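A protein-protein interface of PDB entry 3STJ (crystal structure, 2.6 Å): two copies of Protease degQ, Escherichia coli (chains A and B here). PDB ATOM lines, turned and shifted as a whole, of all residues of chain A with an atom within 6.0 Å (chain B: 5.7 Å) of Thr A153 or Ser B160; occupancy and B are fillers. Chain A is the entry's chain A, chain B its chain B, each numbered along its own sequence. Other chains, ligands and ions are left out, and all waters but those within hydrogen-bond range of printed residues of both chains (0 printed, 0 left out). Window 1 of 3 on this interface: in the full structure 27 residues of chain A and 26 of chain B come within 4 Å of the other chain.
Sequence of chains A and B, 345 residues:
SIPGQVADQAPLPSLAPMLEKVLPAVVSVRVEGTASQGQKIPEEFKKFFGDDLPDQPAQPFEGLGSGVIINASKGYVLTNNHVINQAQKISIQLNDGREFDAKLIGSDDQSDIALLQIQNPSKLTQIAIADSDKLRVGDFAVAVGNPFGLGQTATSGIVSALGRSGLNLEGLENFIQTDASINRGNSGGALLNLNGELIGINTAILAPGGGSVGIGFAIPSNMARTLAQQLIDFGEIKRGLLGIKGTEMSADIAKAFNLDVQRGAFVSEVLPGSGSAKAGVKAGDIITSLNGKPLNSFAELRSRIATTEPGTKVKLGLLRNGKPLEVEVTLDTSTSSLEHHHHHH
O of Gly A145 is in hydrogen-bond range of N of Thr A153, 2.9 Å away.
O of Gly A151 lies within hydrogen-bond range of OG1 of Thr A153 (3.3 Å).
ND2 of Asn A146 sits close to N of Leu A150, at 3.5 Å.
N of Ser B160 lies within hydrogen-bond range of O of Gln B177.
NE of Arg B164 sits at hydrogen-bond distance from OE1 of Gln B177.
O of Ala A143 sits at hydrogen-bond distance from N of Thr A155.
No position is printed for both chains.
Of the 16 pairs that touch across the chains among the printed residues, none has its exchanged pair printed and touching as well.
Hydrophobic or aromatic side chains of chain B within 4 Å of the printed part of chain A: Val B137, Ile B158, Ala B161 and Ile B215.
Pro A147 touches Ile B215 (CG to CD1, 3.7 Å).
Leu A150 touches Gln B177.
Ile B215 touches Leu A150 (CG2 to CD1, 3.5 Å).
O of Ser B160 touches O of Gln A152 (3.9 Å).
O of Gln A152 touches CB of Ala B161, 3.7 Å away.
Thr A153 touches Ser B160 (CA to O, 3.6 Å).
Ala A154 touches Val B137.
O of Ala A154 touches CD1 of Ile B158, 3.4 Å away.
Thr A155 touches Ser B160 (CG2 to OG, 3.9999 Å).
Thr A155 touches Asp B179 (CA to OD2, 3.6 Å).
The backbone carbonyl oxygen of Leu A150 sits close to the guanidinium group of Arg B164 (3.5 Å).
The side-chain hydroxyl (OG1) of Thr A153 lies within hydrogen-bond range of the guanidinium group (NH2) of Arg B164 (2.8 Å).
The backbone carbonyl oxygen (O) of Gln A152 sits at hydrogen-bond distance from the guanidinium group (NH2) of Arg B164, at 3.2 Å.
The side-chain hydroxyl (OG1) of Thr A153 sits at hydrogen-bond distance from the side-chain amide nitrogen (NE2) of Gln B177.
The side-chain hydroxyl (OG) of Ser B160 is in hydrogen-bond range of the backbone carbonyl oxygen (O) of Ala A154.
The backbone carbonyl oxygen of Gly A151 lies within hydrogen-bond range of the guanidinium group of Arg B164 (3.1 Å).
Thr A153 touches three residues of chain B.
Of the printed residues of chain A, Ser B160 touches Gln A152, Thr A153, Ala A154 and Thr A155.
Printed residues of chain B within 4 Å of Gln A152: Ser B160, Ala B161 and Arg B164.
Of the printed residues of chain A, Ile B158 touches Ala A154 (3.4 Å).
Of the printed residues of chain B, Leu A150 touches Arg B164, Gln B177 and Ile B215.
Printed residues of chain A within 4 Å of Ile B215: Pro A147 and Leu A150.
Of the printed residues of chain B, Thr A155 touches Ser B160 (3.9999 Å) and Asp B179 (3.6 Å).
Asn A186 touches none of the printed residues of chain B.
The nearest residue of chain B that does not touch Thr A153 is Ile B215 (4.5 Å).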
ATOM      1  N   ALA A 143      25.220  17.265 -21.169  1.00  0.00           N
ATOM      2  CA  ALA A 143      23.951  17.817 -21.631  1.00  0.00           C
ATOM      3  C   ALA A 143      22.862  16.710 -21.578  1.00  0.00           C
ATOM      4  O   ALA A 143      23.084  15.597 -22.063  1.00  0.00           O
ATOM      5  CB  ALA A 143      24.115  18.365 -23.036  1.00  0.00           C
ATOM      6  N   VAL A 144      21.744  16.971 -20.906  1.00  0.00           N
ATOM      7  CA  VAL A 144      20.676  15.968 -20.725  1.00  0.00           C
ATOM      8  C   VAL A 144      19.341  16.573 -21.207  1.00  0.00           C
ATOM      9  O   VAL A 144      18.962  17.670 -20.813  1.00  0.00           O
ATOM     10  CB  VAL A 144      20.596  15.433 -19.258  1.00  0.00           C
ATOM     11  CG1 VAL A 144      19.558  14.311 -19.127  1.00  0.00           C
ATOM     12  CG2 VAL A 144      21.964  14.973 -18.739  1.00  0.00           C
ATOM     13  N   GLY A 145      18.689  15.864 -22.103  1.00  0.00           N
ATOM     14  CA  GLY A 145      17.447  16.300 -22.719  1.00  0.00           C
ATOM     15  C   GLY A 145      16.822  15.273 -23.645  1.00  0.00           C
ATOM     16  O   GLY A 145      17.185  14.088 -23.644  1.00  0.00           O
ATOM     17  N   ASN A 146      15.900  15.757 -24.487  1.00  0.00           N
ATOM     18  CA  ASN A 146      15.064  14.975 -25.386  1.00  0.00           C
ATOM     19  C   ASN A 146      15.213  15.366 -26.851  1.00  0.00           C
ATOM     20  O   ASN A 146      14.229  15.824 -27.454  1.00  0.00           O
ATOM     21  CB  ASN A 146      13.622  15.210 -24.962  1.00  0.00           C
ATOM     22  CG  ASN A 146      12.913  13.948 -24.690  1.00  0.00           C
ATOM     23  OD1 ASN A 146      12.857  13.499 -23.538  1.00  0.00           O
ATOM     24  ND2 ASN A 146      12.425  13.323 -25.758  1.00  0.00           N
ATOM     25  N   PRO A 147      16.387  15.176 -27.492  1.00  0.00           N
ATOM     26  CA  PRO A 147      16.489  15.579 -28.898  1.00  0.00           C
ATOM     27  C   PRO A 147      15.639  14.682 -29.761  1.00  0.00           C
ATOM     28  O   PRO A 147      15.586  13.471 -29.506  1.00  0.00           O
ATOM     29  CB  PRO A 147      17.979  15.451 -29.209  1.00  0.00           C
ATOM     30  CG  PRO A 147      18.496  14.503 -28.198  1.00  0.00           C
ATOM     31  CD  PRO A 147      17.669  14.646 -26.985  1.00  0.00           C
ATOM     32  N   LEU A 150      13.268  11.543 -28.637  1.00  0.00           N
ATOM     33  CA  LEU A 150      13.695  10.132 -28.518  1.00  0.00           C
ATOM     34  C   LEU A 150      13.485   9.547 -27.131  1.00  0.00           C
ATOM     35  O   LEU A 150      13.291   8.330 -26.973  1.00  0.00           O
ATOM     36  CB  LEU A 150      15.175   9.966 -28.897  1.00  0.00           C
ATOM     37  CG  LEU A 150      15.536  10.233 -30.325  1.00  0.00           C
ATOM     38  CD1 LEU A 150      17.005  10.507 -30.466  1.00  0.00           C
ATOM     39  CD2 LEU A 150      15.105   9.079 -31.202  1.00  0.00           C
ATOM     40  N   GLY A 151      13.553  10.414 -26.152  1.00  0.00           N
ATOM     41  CA  GLY A 151      13.531  10.038 -24.752  1.00  0.00           C
ATOM     42  C   GLY A 151      14.790  10.652 -24.178  1.00  0.00           C
ATOM     43  O   GLY A 151      15.546  11.311 -24.912  1.00  0.00           O
ATOM     44  N   GLN A 152      15.031  10.434 -22.882  1.00  0.00           N
ATOM     45  CA  GLN A 152      16.204  10.980 -22.195  1.00  0.00           C
ATOM     46  C   GLN A 152      17.526  10.498 -22.839  1.00  0.00           C
ATOM     47  O   GLN A 152      17.805   9.284 -22.960  1.00  0.00           O
ATOM     48  CB  GLN A 152      16.185  10.643 -20.713  1.00  0.00           C
ATOM     49  CG  GLN A 152      17.159  11.507 -19.947  1.00  0.00           C
ATOM     50  CD  GLN A 152      16.887  11.427 -18.485  1.00  0.00           C
ATOM     51  OE1 GLN A 152      16.299  12.345 -17.873  1.00  0.00           O
ATOM     52  NE2 GLN A 152      17.306  10.313 -17.904  1.00  0.00           N
ATOM     53  N   THR A 153      18.297  11.482 -23.272  1.00  0.00           N
ATOM     54  CA  THR A 153      19.582  11.360 -23.925  1.00  0.00           C
ATOM     55  C   THR A 153      20.599  12.186 -23.182  1.00  0.00           C
ATOM     56  O   THR A 153      20.341  13.361 -22.883  1.00  0.00           O
ATOM     57  CB  THR A 153      19.436  11.833 -25.354  1.00  0.00           C
ATOM     58  OG1 THR A 153      18.588  10.919 -26.042  1.00  0.00           O
ATOM     59  CG2 THR A 153      20.763  11.997 -26.072  1.00  0.00           C
ATOM     60  N   ALA A 154      21.757  11.579 -22.898  1.00  0.00           N
ATOM     61  CA  ALA A 154      22.896  12.248 -22.255  1.00  0.00           C
ATOM     62  C   ALA A 154      24.022  12.429 -23.268  1.00  0.00           C
ATOM     63  O   ALA A 154      24.358  11.473 -23.973  1.00  0.00           O
ATOM     64  CB  ALA A 154      23.380  11.431 -21.070  1.00  0.00           C
ATOM     65  N   THR A 155      24.576  13.649 -23.398  1.00  0.00           N
ATOM     66  CA  THR A 155      25.685  13.860 -24.329  1.00  0.00           C
ATOM     67  C   THR A 155      26.787  14.540 -23.576  1.00  0.00           C
ATOM     68  O   THR A 155      26.505  15.214 -22.603  1.00  0.00           O
ATOM     69  CB  THR A 155      25.269  14.578 -25.611  1.00  0.00           C
ATOM     70  OG1 THR A 155      24.681  15.842 -25.309  1.00  0.00           O
ATOM     71  CG2 THR A 155      24.372  13.718 -26.499  1.00  0.00           C
ATOM     72  N   ASN A 186      16.272  19.504 -27.035  1.00  0.00           N
ATOM     73  CA  ASN A 186      17.169  19.628 -25.885  1.00  0.00           C
ATOM     74  C   ASN A 186      16.861  20.873 -25.054  1.00  0.00           C
ATOM     75  O   ASN A 186      17.276  20.941 -23.902  1.00  0.00           O
ATOM     76  CB  ASN A 186      18.622  19.699 -26.379  1.00  0.00           C
ATOM     77  CG  ASN A 186      19.358  18.408 -26.361  1.00  0.00           C
ATOM     78  OD1 ASN A 186      19.652  17.846 -25.316  1.00  0.00           O
ATOM     79  ND2 ASN A 186      19.756  17.961 -27.515  1.00  0.00           N
ATOM     80  N   VAL B 137      24.114   4.340 -19.048  1.00  0.00           N
ATOM     81  CA  VAL B 137      24.194   5.687 -19.621  1.00  0.00           C
ATOM     82  C   VAL B 137      25.330   6.414 -18.889  1.00  0.00           C
ATOM     83  O   VAL B 137      25.327   6.474 -17.664  1.00  0.00           O
ATOM     84  CB  VAL B 137      22.833   6.431 -19.531  1.00  0.00           C
ATOM     85  CG1 VAL B 137      22.977   7.887 -19.934  1.00  0.00           C
ATOM     86  CG2 VAL B 137      21.773   5.734 -20.363  1.00  0.00           C
ATOM     87  N   GLY B 138      26.310   6.870 -19.641  1.00  0.00           N
ATOM     88  CA  GLY B 138      27.466   7.543 -19.082  1.00  0.00           C
ATOM     89  C   GLY B 138      28.759   6.824 -19.359  1.00  0.00           C
ATOM     90  O   GLY B 138      29.821   7.455 -19.314  1.00  0.00           O
ATOM     91  N   ILE B 158      30.029   8.864 -25.403  1.00  0.00           N
ATOM     92  CA  ILE B 158      29.445   8.150 -24.258  1.00  0.00           C
ATOM     93  C   ILE B 158      28.248   7.345 -24.710  1.00  0.00           C
ATOM     94  O   ILE B 158      27.771   7.540 -25.834  1.00  0.00           O
ATOM     95  CB  ILE B 158      29.044   9.092 -23.079  1.00  0.00           C
ATOM     96  CG1 ILE B 158      27.977  10.133 -23.488  1.00  0.00           C
ATOM     97  CG2 ILE B 158      30.262   9.706 -22.369  1.00  0.00           C
ATOM     98  CD1 ILE B 158      27.185  10.747 -22.287  1.00  0.00           C
ATOM     99  N   VAL B 159      27.746   6.446 -23.808  1.00  0.00           N
ATOM    100  CA  VAL B 159      26.486   5.730 -24.001  1.00  0.00           C
ATOM    101  C   VAL B 159      25.443   6.735 -23.573  1.00  0.00           C
ATOM    102  O   VAL B 159      25.455   7.156 -22.419  1.00  0.00           O
ATOM    103  CB  VAL B 159      26.393   4.374 -23.265  1.00  0.00           C
ATOM    104  CG1 VAL B 159      24.984   3.796 -23.338  1.00  0.00           C
ATOM    105  CG2 VAL B 159      27.410   3.387 -23.814  1.00  0.00           C
ATOM    106  N   SER B 160      24.676   7.259 -24.553  1.00  0.00           N
ATOM    107  CA  SER B 160      23.667   8.312 -24.394  1.00  0.00           C
ATOM    108  C   SER B 160      22.326   7.780 -23.902  1.00  0.00           C
ATOM    109  O   SER B 160      21.632   8.479 -23.169  1.00  0.00           O
ATOM    110  CB  SER B 160      23.454   9.008 -25.724  1.00  0.00           C
ATOM    111  OG  SER B 160      24.615   9.753 -26.031  1.00  0.00           O
ATOM    112  N   ALA B 161      21.952   6.558 -24.336  1.00  0.00           N
ATOM    113  CA  ALA B 161      20.690   5.887 -24.018  1.00  0.00           C
ATOM    114  C   ALA B 161      20.802   4.414 -24.334  1.00  0.00           C
ATOM    115  O   ALA B 161      21.730   3.992 -25.034  1.00  0.00           O
ATOM    116  CB  ALA B 161      19.541   6.519 -24.797  1.00  0.00           C
ATOM    117  N   LEU B 162      19.879   3.618 -23.805  1.00  0.00           N
ATOM    118  CA  LEU B 162      19.855   2.148 -23.977  1.00  0.00           C
ATOM    119  C   LEU B 162      18.439   1.664 -24.225  1.00  0.00           C
ATOM    120  O   LEU B 162      17.491   2.340 -23.806  1.00  0.00           O
ATOM    121  CB  LEU B 162      20.414   1.465 -22.731  1.00  0.00           C
ATOM    122  CG  LEU B 162      21.907   1.685 -22.458  1.00  0.00           C
ATOM    123  CD1 LEU B 162      22.206   1.500 -21.005  1.00  0.00           C
ATOM    124  CD2 LEU B 162      22.805   0.783 -23.357  1.00  0.00           C
ATOM    125  N   ARG B 164      16.703   1.467 -27.043  1.00  0.00           N
ATOM    126  CA  ARG B 164      15.984   2.371 -27.938  1.00  0.00           C
ATOM    127  C   ARG B 164      15.245   1.646 -29.044  1.00  0.00           C
ATOM    128  O   ARG B 164      15.848   0.925 -29.840  1.00  0.00           O
ATOM    129  CB  ARG B 164      16.943   3.413 -28.544  1.00  0.00           C
ATOM    130  CG  ARG B 164      17.222   4.584 -27.633  1.00  0.00           C
ATOM    131  CD  ARG B 164      16.023   5.503 -27.486  1.00  0.00           C
ATOM    132  NE  ARG B 164      16.454   6.876 -27.256  1.00  0.00           N
ATOM    133  CZ  ARG B 164      16.508   7.453 -26.068  1.00  0.00           C
ATOM    134  NH1 ARG B 164      16.113   6.797 -24.990  1.00  0.00           N
ATOM    135  NH2 ARG B 164      16.941   8.693 -25.949  1.00  0.00           N
ATOM    136  N   GLN B 177      22.330   4.026 -27.845  1.00  0.00           N
ATOM    137  CA  GLN B 177      22.466   5.339 -28.461  1.00  0.00           C
ATOM    138  C   GLN B 177      23.802   5.946 -27.995  1.00  0.00           C
ATOM    139  O   GLN B 177      24.148   5.826 -26.820  1.00  0.00           O
ATOM    140  CB  GLN B 177      21.264   6.217 -28.122  1.00  0.00           C
ATOM    141  CG  GLN B 177      21.188   7.461 -28.985  1.00  0.00           C
ATOM    142  CD  GLN B 177      20.062   8.317 -28.550  1.00  0.00           C
ATOM    143  OE1 GLN B 177      18.926   7.862 -28.406  1.00  0.00           O
ATOM    144  NE2 GLN B 177      20.360   9.568 -28.303  1.00  0.00           N
ATOM    145  N   THR B 178      24.558   6.574 -28.913  1.00  0.00           N
ATOM    146  CA  THR B 178      25.868   7.135 -28.564  1.00  0.00           C
ATOM    147  C   THR B 178      26.075   8.469 -29.239  1.00  0.00           C
ATOM    148  O   THR B 178      25.480   8.720 -30.269  1.00  0.00           O
ATOM    149  CB  THR B 178      27.020   6.129 -28.889  1.00  0.00           C
ATOM    150  OG1 THR B 178      28.268   6.705 -28.540  1.00  0.00           O
ATOM    151  CG2 THR B 178      27.057   5.697 -30.365  1.00  0.00           C
ATOM    152  N   ASP B 179      26.913   9.323 -28.666  1.00  0.00           N
ATOM    153  CA  ASP B 179      27.218  10.637 -29.248  1.00  0.00           C
ATOM    154  C   ASP B 179      28.594  10.610 -29.951  1.00  0.00           C
ATOM    155  O   ASP B 179      29.049  11.645 -30.441  1.00  0.00           O
ATOM    156  CB  ASP B 179      27.104  11.799 -28.224  1.00  0.00           C
ATOM    157  CG  ASP B 179      28.119  11.835 -27.097  1.00  0.00           C
ATOM    158  OD1 ASP B 179      28.673  10.760 -26.760  1.00  0.00           O
ATOM    159  OD2 ASP B 179      28.330  12.939 -26.516  1.00  0.00           O
ATOM    160  N   GLY B 214      25.504  13.729 -33.469  1.00  0.00           N
ATOM    161  CA  GLY B 214      25.695  13.053 -32.186  1.00  0.00           C
ATOM    162  C   GLY B 214      24.560  12.150 -31.704  1.00  0.00           C
ATOM    163  O   GLY B 214      24.450  11.896 -30.502  1.00  0.00           O
ATOM    164  N   ILE B 215      23.710  11.646 -32.630  1.00  0.00           N
ATOM    165  CA  ILE B 215      22.625  10.710 -32.330  1.00  0.00           C
ATOM    166  C   ILE B 215      22.834   9.482 -33.195  1.00  0.00           C
ATOM    167  O   ILE B 215      22.355   9.435 -34.344  1.00  0.00           O
ATOM    168  CB  ILE B 215      21.198  11.320 -32.530  1.00  0.00           C
ATOM    169  CG1 ILE B 215      21.035  12.773 -31.963  1.00  0.00           C
ATOM    170  CG2 ILE B 215      20.102  10.340 -32.078  1.00  0.00           C
ATOM    171  CD1 ILE B 215      20.833  12.898 -30.520  1.00  0.00           C
